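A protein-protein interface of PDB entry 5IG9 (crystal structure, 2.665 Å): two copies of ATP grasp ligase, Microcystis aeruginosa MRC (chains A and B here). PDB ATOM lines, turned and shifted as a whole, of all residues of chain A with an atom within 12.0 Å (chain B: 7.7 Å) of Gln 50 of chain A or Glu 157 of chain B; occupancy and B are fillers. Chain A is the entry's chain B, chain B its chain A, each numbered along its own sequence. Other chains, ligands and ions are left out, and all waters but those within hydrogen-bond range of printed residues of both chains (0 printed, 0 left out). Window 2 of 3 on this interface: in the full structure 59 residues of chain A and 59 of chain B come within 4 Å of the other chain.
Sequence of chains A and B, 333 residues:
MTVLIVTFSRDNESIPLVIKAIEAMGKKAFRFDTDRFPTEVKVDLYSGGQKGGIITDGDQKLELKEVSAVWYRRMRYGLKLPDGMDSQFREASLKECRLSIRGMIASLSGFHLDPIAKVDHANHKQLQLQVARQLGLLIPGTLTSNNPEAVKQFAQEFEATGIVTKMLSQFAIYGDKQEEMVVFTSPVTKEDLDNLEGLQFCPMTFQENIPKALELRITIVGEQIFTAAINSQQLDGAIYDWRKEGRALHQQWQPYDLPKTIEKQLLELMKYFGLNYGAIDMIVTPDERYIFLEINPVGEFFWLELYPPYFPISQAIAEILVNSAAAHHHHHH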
ATOM      1  N   ASP A  44     -30.035 -16.979 -23.838  1.00  0.00           N
ATOM      2  CA  ASP A  44     -28.787 -16.819 -24.578  1.00  0.00           C
ATOM      3  C   ASP A  44     -28.827 -15.452 -25.240  1.00  0.00           C
ATOM      4  O   ASP A  44     -29.602 -15.244 -26.175  1.00  0.00           O
ATOM      5  CB  ASP A  44     -28.612 -17.923 -25.621  1.00  0.00           C
ATOM      6  CG  ASP A  44     -28.549 -19.303 -25.007  1.00  0.00           C
ATOM      7  OD1 ASP A  44     -27.882 -19.460 -23.964  1.00  0.00           O
ATOM      8  OD2 ASP A  44     -29.172 -20.230 -25.568  1.00  0.00           O
ATOM      9  N   LEU A  45     -28.001 -14.527 -24.761  1.00  0.00           N
ATOM     10  CA  LEU A  45     -28.008 -13.143 -25.223  1.00  0.00           C
ATOM     11  C   LEU A  45     -26.724 -12.883 -26.002  1.00  0.00           C
ATOM     12  O   LEU A  45     -25.635 -12.839 -25.419  1.00  0.00           O
ATOM     13  CB  LEU A  45     -28.151 -12.181 -24.045  1.00  0.00           C
ATOM     14  CG  LEU A  45     -29.363 -12.437 -23.142  1.00  0.00           C
ATOM     15  CD1 LEU A  45     -29.367 -11.525 -21.928  1.00  0.00           C
ATOM     16  CD2 LEU A  45     -30.650 -12.291 -23.932  1.00  0.00           C
ATOM     17  N   TYR A  46     -26.854 -12.712 -27.314  1.00  0.00           N
ATOM     18  CA  TYR A  46     -25.717 -12.510 -28.197  1.00  0.00           C
ATOM     19  C   TYR A  46     -25.579 -11.034 -28.541  1.00  0.00           C
ATOM     20  O   TYR A  46     -26.571 -10.353 -28.815  1.00  0.00           O
ATOM     21  CB  TYR A  46     -25.866 -13.326 -29.484  1.00  0.00           C
ATOM     22  CG  TYR A  46     -25.839 -14.823 -29.277  1.00  0.00           C
ATOM     23  CD1 TYR A  46     -24.637 -15.514 -29.239  1.00  0.00           C
ATOM     24  CD2 TYR A  46     -27.016 -15.547 -29.128  1.00  0.00           C
ATOM     25  CE1 TYR A  46     -24.604 -16.883 -29.054  1.00  0.00           C
ATOM     26  CE2 TYR A  46     -26.993 -16.919 -28.940  1.00  0.00           C
ATOM     27  CZ  TYR A  46     -25.783 -17.582 -28.906  1.00  0.00           C
ATOM     28  OH  TYR A  46     -25.750 -18.947 -28.722  1.00  0.00           O
ATOM     29  N   SER A  47     -24.342 -10.548 -28.526  1.00  0.00           N
ATOM     30  CA  SER A  47     -24.028  -9.177 -28.896  1.00  0.00           C
ATOM     31  C   SER A  47     -22.913  -9.192 -29.929  1.00  0.00           C
ATOM     32  O   SER A  47     -21.972  -9.984 -29.828  1.00  0.00           O
ATOM     33  CB  SER A  47     -23.614  -8.345 -27.674  1.00  0.00           C
ATOM     34  OG  SER A  47     -24.718  -8.119 -26.815  1.00  0.00           O
ATOM     35  N   GLY A  48     -23.023  -8.318 -30.924  1.00  0.00           N
ATOM     36  CA  GLY A  48     -22.019  -8.259 -31.963  1.00  0.00           C
ATOM     37  C   GLY A  48     -22.595  -8.552 -33.329  1.00  0.00           C
ATOM     38  O   GLY A  48     -23.795  -8.366 -33.555  1.00  0.00           O
ATOM     39  N   GLY A  49     -21.748  -9.014 -34.251  1.00  0.00           N
ATOM     40  CA  GLY A  49     -22.228  -9.339 -35.582  1.00  0.00           C
ATOM     41  C   GLY A  49     -23.191 -10.507 -35.597  1.00  0.00           C
ATOM     42  O   GLY A  49     -23.986 -10.648 -36.530  1.00  0.00           O
ATOM     43  N   GLN A  50     -23.145 -11.351 -34.568  1.00  0.00           N
ATOM     44  CA  GLN A  50     -24.000 -12.530 -34.510  1.00  0.00           C
ATOM     45  C   GLN A  50     -25.426 -12.162 -34.111  1.00  0.00           C
ATOM     46  O   GLN A  50     -25.896 -11.055 -34.396  1.00  0.00           O
ATOM     47  CB  GLN A  50     -23.421 -13.565 -33.539  1.00  0.00           C
ATOM     48  CG  GLN A  50     -22.092 -14.184 -33.981  1.00  0.00           C
ATOM     49  CD  GLN A  50     -22.267 -15.401 -34.877  1.00  0.00           C
ATOM     50  OE1 GLN A  50     -22.876 -15.323 -35.944  1.00  0.00           O
ATOM     51  NE2 GLN A  50     -21.733 -16.537 -34.440  1.00  0.00           N
ATOM     52  N   LYS A  51     -26.106 -13.079 -33.433  1.00  0.00           N
ATOM     53  CA  LYS A  51     -27.551 -13.002 -33.248  1.00  0.00           C
ATOM     54  C   LYS A  51     -27.923 -11.935 -32.219  1.00  0.00           C
ATOM     55  O   LYS A  51     -27.097 -11.144 -31.756  1.00  0.00           O
ATOM     56  CB  LYS A  51     -28.104 -14.361 -32.830  1.00  0.00           C
ATOM     57  CG  LYS A  51     -28.207 -15.379 -33.946  1.00  0.00           C
ATOM     58  CD  LYS A  51     -26.897 -16.119 -34.140  1.00  0.00           C
ATOM     59  CE  LYS A  51     -26.472 -16.825 -32.865  1.00  0.00           C
ATOM     60  NZ  LYS A  51     -25.278 -17.685 -33.080  1.00  0.00           N
ATOM     61  N   GLY A  52     -29.207 -11.914 -31.868  1.00  0.00           N
ATOM     62  CA  GLY A  52     -29.708 -11.142 -30.751  1.00  0.00           C
ATOM     63  C   GLY A  52     -29.851 -12.011 -29.519  1.00  0.00           C
ATOM     64  O   GLY A  52     -29.159 -11.791 -28.520  1.00  0.00           O
ATOM     65  N   GLY A  53     -30.726 -13.008 -29.575  1.00  0.00           N
ATOM     66  CA  GLY A  53     -30.856 -13.926 -28.462  1.00  0.00           C
ATOM     67  C   GLY A  53     -32.039 -14.856 -28.621  1.00  0.00           C
ATOM     68  O   GLY A  53     -32.864 -14.711 -29.528  1.00  0.00           O
ATOM     69  N   ILE A  54     -32.104 -15.822 -27.703  1.00  0.00           N
ATOM     70  CA  ILE A  54     -33.189 -16.800 -27.656  1.00  0.00           C
ATOM     71  C   ILE A  54     -33.450 -17.171 -26.200  1.00  0.00           C
ATOM     72  O   ILE A  54     -32.524 -17.238 -25.385  1.00  0.00           O
ATOM     73  CB  ILE A  54     -32.865 -18.055 -28.499  1.00  0.00           C
ATOM     74  CG1 ILE A  54     -34.008 -19.075 -28.439  1.00  0.00           C
ATOM     75  CG2 ILE A  54     -31.571 -18.703 -28.035  1.00  0.00           C
ATOM     76  CD1 ILE A  54     -33.754 -20.317 -29.262  1.00  0.00           C
ATOM     77  N   GLU A  63     -37.390 -16.653 -29.994  1.00  0.00           N
ATOM     78  CA  GLU A  63     -36.322 -15.898 -30.631  1.00  0.00           C
ATOM     79  C   GLU A  63     -36.591 -14.417 -30.400  1.00  0.00           C
ATOM     80  O   GLU A  63     -37.634 -13.902 -30.816  1.00  0.00           O
ATOM     81  CB  GLU A  63     -36.236 -16.219 -32.122  1.00  0.00           C
ATOM     82  CG  GLU A  63     -35.696 -17.610 -32.422  1.00  0.00           C
ATOM     83  CD  GLU A  63     -35.339 -17.795 -33.885  1.00  0.00           C
ATOM     84  OE1 GLU A  63     -35.891 -18.716 -34.524  1.00  0.00           O
ATOM     85  OE2 GLU A  63     -34.508 -17.015 -34.398  1.00  0.00           O
ATOM     86  N   LEU A  64     -35.659 -13.738 -29.728  1.00  0.00           N
ATOM     87  CA  LEU A  64     -35.858 -12.338 -29.368  1.00  0.00           C
ATOM     88  C   LEU A  64     -36.038 -11.430 -30.576  1.00  0.00           C
ATOM     89  O   LEU A  64     -36.419 -10.266 -30.402  1.00  0.00           O
ATOM     90  CB  LEU A  64     -34.686 -11.844 -28.524  1.00  0.00           C
ATOM     91  CG  LEU A  64     -34.479 -12.579 -27.202  1.00  0.00           C
ATOM     92  CD1 LEU A  64     -33.298 -11.989 -26.452  1.00  0.00           C
ATOM     93  CD2 LEU A  64     -35.743 -12.526 -26.357  1.00  0.00           C
ATOM     94  N   LYS A  65     -35.771 -11.920 -31.787  1.00  0.00           N
ATOM     95  CA  LYS A  65     -36.003 -11.114 -32.980  1.00  0.00           C
ATOM     96  C   LYS A  65     -37.490 -10.940 -33.250  1.00  0.00           C
ATOM     97  O   LYS A  65     -37.898  -9.949 -33.869  1.00  0.00           O
ATOM     98  CB  LYS A  65     -35.322 -11.753 -34.194  1.00  0.00           C
ATOM     99  CG  LYS A  65     -33.809 -11.543 -34.279  1.00  0.00           C
ATOM    100  CD  LYS A  65     -33.052 -12.257 -33.164  1.00  0.00           C
ATOM    101  CE  LYS A  65     -33.382 -13.743 -33.116  1.00  0.00           C
ATOM    102  NZ  LYS A  65     -32.837 -14.384 -31.887  1.00  0.00           N
ATOM    103  N   SER A 107     -32.339  -3.737 -24.004  1.00  0.00           N
ATOM    104  CA  SER A 107     -31.833  -3.789 -25.373  1.00  0.00           C
ATOM    105  C   SER A 107     -32.938  -4.052 -26.387  1.00  0.00           C
ATOM    106  O   SER A 107     -32.824  -3.635 -27.546  1.00  0.00           O
ATOM    107  CB  SER A 107     -30.755  -4.869 -25.493  1.00  0.00           C
ATOM    108  OG  SER A 107     -29.674  -4.613 -24.615  1.00  0.00           O
ATOM    109  N   ARG B 133     -22.490  -0.567 -31.617  1.00  0.00           N
ATOM    110  CA  ARG B 133     -22.445  -1.237 -32.913  1.00  0.00           C
ATOM    111  C   ARG B 133     -23.384  -0.577 -33.916  1.00  0.00           C
ATOM    112  O   ARG B 133     -23.054  -0.469 -35.102  1.00  0.00           O
ATOM    113  CB  ARG B 133     -22.788  -2.716 -32.750  1.00  0.00           C
ATOM    114  CG  ARG B 133     -22.695  -3.520 -34.028  1.00  0.00           C
ATOM    115  CD  ARG B 133     -22.989  -4.986 -33.775  1.00  0.00           C
ATOM    116  NE  ARG B 133     -22.985  -5.757 -35.012  1.00  0.00           N
ATOM    117  CZ  ARG B 133     -24.063  -5.994 -35.749  1.00  0.00           C
ATOM    118  NH1 ARG B 133     -25.244  -5.522 -35.372  1.00  0.00           N
ATOM    119  NH2 ARG B 133     -23.961  -6.704 -36.865  1.00  0.00           N
ATOM    120  N   GLY B 141     -17.470 -10.181 -30.045  1.00  0.00           N
ATOM    121  CA  GLY B 141     -18.546 -11.150 -29.926  1.00  0.00           C
ATOM    122  C   GLY B 141     -18.831 -11.483 -28.474  1.00  0.00           C
ATOM    123  O   GLY B 141     -17.948 -11.962 -27.758  1.00  0.00           O
ATOM    124  N   THR B 142     -20.056 -11.236 -28.025  1.00  0.00           N
ATOM    125  CA  THR B 142     -20.404 -11.348 -26.617  1.00  0.00           C
ATOM    126  C   THR B 142     -21.614 -12.254 -26.444  1.00  0.00           C
ATOM    127  O   THR B 142     -22.579 -12.171 -27.208  1.00  0.00           O
ATOM    128  CB  THR B 142     -20.676  -9.963 -26.013  1.00  0.00           C
ATOM    129  OG1 THR B 142     -19.522  -9.136 -26.181  1.00  0.00           O
ATOM    130  CG2 THR B 142     -21.004 -10.072 -24.537  1.00  0.00           C
ATOM    131  N   ALA B 150     -24.828 -23.528 -25.714  1.00  0.00           N
ATOM    132  CA  ALA B 150     -24.534 -22.279 -26.407  1.00  0.00           C
ATOM    133  C   ALA B 150     -23.132 -21.784 -26.076  1.00  0.00           C
ATOM    134  O   ALA B 150     -22.455 -21.202 -26.930  1.00  0.00           O
ATOM    135  CB  ALA B 150     -25.576 -21.221 -26.049  1.00  0.00           C
ATOM    136  N   VAL B 151     -22.681 -22.011 -24.842  1.00  0.00           N
ATOM    137  CA  VAL B 151     -21.348 -21.577 -24.440  1.00  0.00           C
ATOM    138  C   VAL B 151     -20.276 -22.422 -25.119  1.00  0.00           C
ATOM    139  O   VAL B 151     -19.264 -21.892 -25.592  1.00  0.00           O
ATOM    140  CB  VAL B 151     -21.220 -21.614 -22.907  1.00  0.00           C
ATOM    141  CG1 VAL B 151     -19.792 -21.301 -22.483  1.00  0.00           C
ATOM    142  CG2 VAL B 151     -22.194 -20.634 -22.278  1.00  0.00           C
ATOM    143  N   LYS B 152     -20.470 -23.744 -25.171  1.00  0.00           N
ATOM    144  CA  LYS B 152     -19.539 -24.600 -25.904  1.00  0.00           C
ATOM    145  C   LYS B 152     -19.456 -24.184 -27.366  1.00  0.00           C
ATOM    146  O   LYS B 152     -18.363 -24.063 -27.934  1.00  0.00           O
ATOM    147  CB  LYS B 152     -19.967 -26.065 -25.798  1.00  0.00           C
ATOM    148  CG  LYS B 152     -19.912 -26.653 -24.401  1.00  0.00           C
ATOM    149  CD  LYS B 152     -18.486 -26.761 -23.879  1.00  0.00           C
ATOM    150  CE  LYS B 152     -17.608 -27.617 -24.782  1.00  0.00           C
ATOM    151  NZ  LYS B 152     -16.819 -26.791 -25.738  1.00  0.00           N
ATOM    152  N   GLN B 153     -20.612 -23.954 -27.988  1.00  0.00           N
ATOM    153  CA  GLN B 153     -20.644 -23.497 -29.371  1.00  0.00           C
ATOM    154  C   GLN B 153     -19.946 -22.150 -29.525  1.00  0.00           C
ATOM    155  O   GLN B 153     -19.291 -21.894 -30.542  1.00  0.00           O
ATOM    156  CB  GLN B 153     -22.095 -23.413 -29.838  1.00  0.00           C
ATOM    157  CG  GLN B 153     -22.303 -23.728 -31.298  1.00  0.00           C
ATOM    158  CD  GLN B 153     -23.752 -24.037 -31.608  1.00  0.00           C
ATOM    159  OE1 GLN B 153     -24.292 -25.053 -31.166  1.00  0.00           O
ATOM    160  NE2 GLN B 153     -24.396 -23.154 -32.363  1.00  0.00           N
ATOM    161  N   PHE B 154     -20.066 -21.280 -28.517  1.00  0.00           N
ATOM    162  CA  PHE B 154     -19.447 -19.959 -28.585  1.00  0.00           C
ATOM    163  C   PHE B 154     -17.932 -20.050 -28.450  1.00  0.00           C
ATOM    164  O   PHE B 154     -17.196 -19.386 -29.188  1.00  0.00           O
ATOM    165  CB  PHE B 154     -20.032 -19.053 -27.499  1.00  0.00           C
ATOM    166  CG  PHE B 154     -19.588 -17.617 -27.591  1.00  0.00           C
ATOM    167  CD1 PHE B 154     -20.188 -16.748 -28.488  1.00  0.00           C
ATOM    168  CD2 PHE B 154     -18.584 -17.135 -26.771  1.00  0.00           C
ATOM    169  CE1 PHE B 154     -19.787 -15.431 -28.572  1.00  0.00           C
ATOM    170  CE2 PHE B 154     -18.180 -15.817 -26.852  1.00  0.00           C
ATOM    171  CZ  PHE B 154     -18.784 -14.966 -27.753  1.00  0.00           C
ATOM    172  N   ALA B 155     -17.447 -20.870 -27.515  1.00  0.00           N
ATOM    173  CA  ALA B 155     -16.004 -21.003 -27.338  1.00  0.00           C
ATOM    174  C   ALA B 155     -15.358 -21.726 -28.514  1.00  0.00           C
ATOM    175  O   ALA B 155     -14.166 -21.532 -28.780  1.00  0.00           O
ATOM    176  CB  ALA B 155     -15.697 -21.739 -26.035  1.00  0.00           C
ATOM    177  N   GLN B 156     -16.124 -22.550 -29.231  1.00  0.00           N
ATOM    178  CA  GLN B 156     -15.560 -23.294 -30.352  1.00  0.00           C
ATOM    179  C   GLN B 156     -15.324 -22.398 -31.562  1.00  0.00           C
ATOM    180  O   GLN B 156     -14.291 -22.515 -32.231  1.00  0.00           O
ATOM    181  CB  GLN B 156     -16.467 -24.466 -30.720  1.00  0.00           C
ATOM    182  CG  GLN B 156     -16.277 -25.704 -29.861  1.00  0.00           C
ATOM    183  CD  GLN B 156     -17.277 -26.797 -30.197  1.00  0.00           C
ATOM    184  OE1 GLN B 156     -18.270 -26.555 -30.887  1.00  0.00           O
ATOM    185  NE2 GLN B 156     -17.020 -28.005 -29.711  1.00  0.00           N
ATOM    186  N   GLU B 157     -16.263 -21.502 -31.869  1.00  0.00           N
ATOM    187  CA  GLU B 157     -16.085 -20.684 -33.065  1.00  0.00           C
ATOM    188  C   GLU B 157     -14.986 -19.643 -32.880  1.00  0.00           C
ATOM    189  O   GLU B 157     -14.427 -19.156 -33.867  1.00  0.00           O
ATOM    190  CB  GLU B 157     -17.401 -20.013 -33.451  1.00  0.00           C
ATOM    191  CG  GLU B 157     -17.855 -18.940 -32.487  1.00  0.00           C
ATOM    192  CD  GLU B 157     -19.183 -18.314 -32.883  1.00  0.00           C
ATOM    193  OE1 GLU B 157     -20.049 -19.036 -33.422  1.00  0.00           O
ATOM    194  OE2 GLU B 157     -19.359 -17.094 -32.656  1.00  0.00           O
ATOM    195  N   PHE B 158     -14.658 -19.298 -31.636  1.00  0.00           N
ATOM    196  CA  PHE B 158     -13.547 -18.408 -31.314  1.00  0.00           C
ATOM    197  C   PHE B 158     -12.396 -19.183 -30.679  1.00  0.00           C
ATOM    198  O   PHE B 158     -11.753 -18.713 -29.740  1.00  0.00           O
ATOM    199  CB  PHE B 158     -13.998 -17.279 -30.388  1.00  0.00           C
ATOM    200  CG  PHE B 158     -15.006 -16.346 -31.005  1.00  0.00           C
ATOM    201  CD1 PHE B 158     -14.624 -15.438 -31.975  1.00  0.00           C
ATOM    202  CD2 PHE B 158     -16.331 -16.363 -30.595  1.00  0.00           C
ATOM    203  CE1 PHE B 158     -15.538 -14.578 -32.538  1.00  0.00           C
ATOM    204  CE2 PHE B 158     -17.254 -15.500 -31.157  1.00  0.00           C
ATOM    205  CZ  PHE B 158     -16.853 -14.605 -32.130  1.00  0.00           C
ATOM    206  N   GLU B 159     -12.125 -20.388 -31.187  1.00  0.00           N
ATOM    207  CA  GLU B 159     -11.093 -21.226 -30.585  1.00  0.00           C
ATOM    208  C   GLU B 159      -9.697 -20.692 -30.876  1.00  0.00           C
ATOM    209  O   GLU B 159      -8.801 -20.805 -30.034  1.00  0.00           O
ATOM    210  CB  GLU B 159     -11.222 -22.665 -31.085  1.00  0.00           C
ATOM    211  CG  GLU B 159     -10.339 -23.669 -30.358  1.00  0.00           C
ATOM    212  CD  GLU B 159     -10.479 -25.074 -30.913  1.00  0.00           C
ATOM    213  OE1 GLU B 159      -9.451 -25.675 -31.289  1.00  0.00           O
ATOM    214  OE2 GLU B 159     -11.622 -25.573 -30.984  1.00  0.00           O
ATOM    215  N   ALA B 160      -9.493 -20.108 -32.060  1.00  0.00           N
ATOM    216  CA  ALA B 160      -8.156 -19.667 -32.451  1.00  0.00           C
ATOM    217  C   ALA B 160      -7.609 -18.627 -31.480  1.00  0.00           C
ATOM    218  O   ALA B 160      -6.487 -18.759 -30.979  1.00  0.00           O
ATOM    219  CB  ALA B 160      -8.182 -19.117 -33.876  1.00  0.00           C
ATOM    220  N   THR B 161      -8.397 -17.591 -31.192  1.00  0.00           N
ATOM    221  CA  THR B 161      -7.980 -16.541 -30.272  1.00  0.00           C
ATOM    222  C   THR B 161      -8.451 -16.778 -28.843  1.00  0.00           C
ATOM    223  O   THR B 161      -7.923 -16.147 -27.920  1.00  0.00           O
ATOM    224  CB  THR B 161      -8.497 -15.178 -30.745  1.00  0.00           C
ATOM    225  OG1 THR B 161      -9.926 -15.166 -30.695  1.00  0.00           O
ATOM    226  CG2 THR B 161      -8.049 -14.897 -32.167  1.00  0.00           C
ATOM    227  N   GLY B 162      -9.421 -17.667 -28.638  1.00  0.00           N
ATOM    228  CA  GLY B 162      -9.938 -17.943 -27.317  1.00  0.00           C
ATOM    229  C   GLY B 162     -11.055 -16.995 -26.929  1.00  0.00           C
ATOM    230  O   GLY B 162     -11.396 -16.050 -27.639  1.00  0.00           O
ATOM    231  N   ILE B 163     -11.653 -17.272 -25.773  1.00  0.00           N
ATOM    232  CA  ILE B 163     -12.649 -16.384 -25.193  1.00  0.00           C
ATOM    233  C   ILE B 163     -12.315 -16.163 -23.726  1.00  0.00           C
ATOM    234  O   ILE B 163     -11.594 -16.944 -23.100  1.00  0.00           O
ATOM    235  CB  ILE B 163     -14.089 -16.921 -25.332  1.00  0.00           C
ATOM    236  CG1 ILE B 163     -14.261 -18.180 -24.488  1.00  0.00           C
ATOM    237  CG2 ILE B 163     -14.432 -17.182 -26.793  1.00  0.00           C
ATOM    238  CD1 ILE B 163     -15.696 -18.549 -24.239  1.00  0.00           C
ATOM    239  N   GLU B 208     -15.419 -12.682 -27.101  1.00  0.00           N
ATOM    240  CA  GLU B 208     -14.310 -12.978 -27.998  1.00  0.00           C
ATOM    241  C   GLU B 208     -13.033 -12.313 -27.503  1.00  0.00           C
ATOM    242  O   GLU B 208     -12.994 -11.098 -27.286  1.00  0.00           O
ATOM    243  CB  GLU B 208     -14.651 -12.494 -29.409  1.00  0.00           C
ATOM    244  CG  GLU B 208     -13.477 -12.414 -30.376  1.00  0.00           C
ATOM    245  CD  GLU B 208     -13.877 -11.806 -31.713  1.00  0.00           C
ATOM    246  OE1 GLU B 208     -14.966 -11.198 -31.784  1.00  0.00           O
ATOM    247  OE2 GLU B 208     -13.109 -11.940 -32.693  1.00  0.00           O
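O of Gly 48 of chain A lies within hydrogen-bond range of NE of Arg 133 of chain B, at 3.1 Å.
The backbone carbonyl oxygen of Thr 142 of chain B sits at hydrogen-bond distance from the backbone NH of Ser 47 of chain A, at 2.7 Å.
OE2 of Glu 157 of chain B lies within hydrogen-bond range of NE2 of Gln 50 of chain A, 3.0 Å away.
The backbone NH of Glu 208 of chain B is in hydrogen-bond range of the backbone carbonyl oxygen of Gly 141 of chain B, 2.7 Å away.
The backbone carbonyl oxygen of Ile 54 of chain A is in hydrogen-bond range of the backbone NH of Asp 44 of chain A.
The backbone carbonyl oxygen of Gly 52 of chain A is in hydrogen-bond range of the backbone NH of Tyr 46 of chain A.
Among the printed residues, merely in contact across the chains: Asp 44 of chain A with Ala 150 of chain B (3.6 Å), Leu 45 of chain A with Thr 142 of chain B (3.6 Å), Tyr 46 of chain A with Thr 142 of chain B (3.3 Å), Tyr 46 of chain A with Ala 150 of chain B (3.5 Å), Ser 47 of chain A with Gly 141 of chain B (3.6 Å) and Gly 49 of chain A with Arg 133 of chain B (3.4 Å).
Of the printed residues of chain B, Leu 45 of chain A touches Thr 142.
Printed residues of chain B within 4 Å of Tyr 46 of chain A: Thr 142 (3.3 Å) and Ala 150 (3.5 Å).
Of the printed residues of chain B, Ser 47 of chain A touches Gly 141 (3.6 Å) and Thr 142 (2.7 Å).
Of the printed residues of chain B, Gly 48 of chain A touches Arg 133.
Gly 49 of chain A touches one residue of chain B.
Gln 50 of chain A touches one residue of chain B.
Gly 141 of chain B touches just one residue of chain A: Ser 47 (3.6 Å).
No residue of chain A comes within 4 Å of Gln 153 of chain B.
No residue of chain A comes within 4 Å of Phe 154 of chain B.
No residue of chain A comes within 4 Å of Ala 155 of chain B.
Glu 157 of chain B touches just one residue of chain A: Gln 50 (3.0 Å).
Phe 158 of chain B touches none of the printed residues of chain A.
Thr 161 of chain B touches none of the printed residues of chain A.
No residue of chain A comes within 4 Å of Gly 162 of chain B.
The nearest residue of chain B that does not touch Gln 50 of chain A is Arg 133 of chain B (5.2 Å).
The nearest residue of chain A that does not touch Glu 157 of chain B is Lys 51 of chain A (5.4 Å).
The nearest printed residue of chain B that does not touch Tyr 46 of chain A is Phe 154 of chain B (4.5 Å).
Of the 15 printed residues of chain A, 7 touch a printed residue of chain B.
Hydrophobic or aromatic side chains of chain A that line the printed part of chain B: Tyr 46.
Along chain B the printed residues that touch a printed residue of chain A span positions 133 to 157.
Among the printed residues, no Asp or Glu carboxylate lies within 4 Å of a Lys or Arg side-chain nitrogen of the other chain.
No position is printed for both chains.
Of the 9 pairs that touch across the chains among the printed residues, none has its exchanged pair printed and touching as well.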
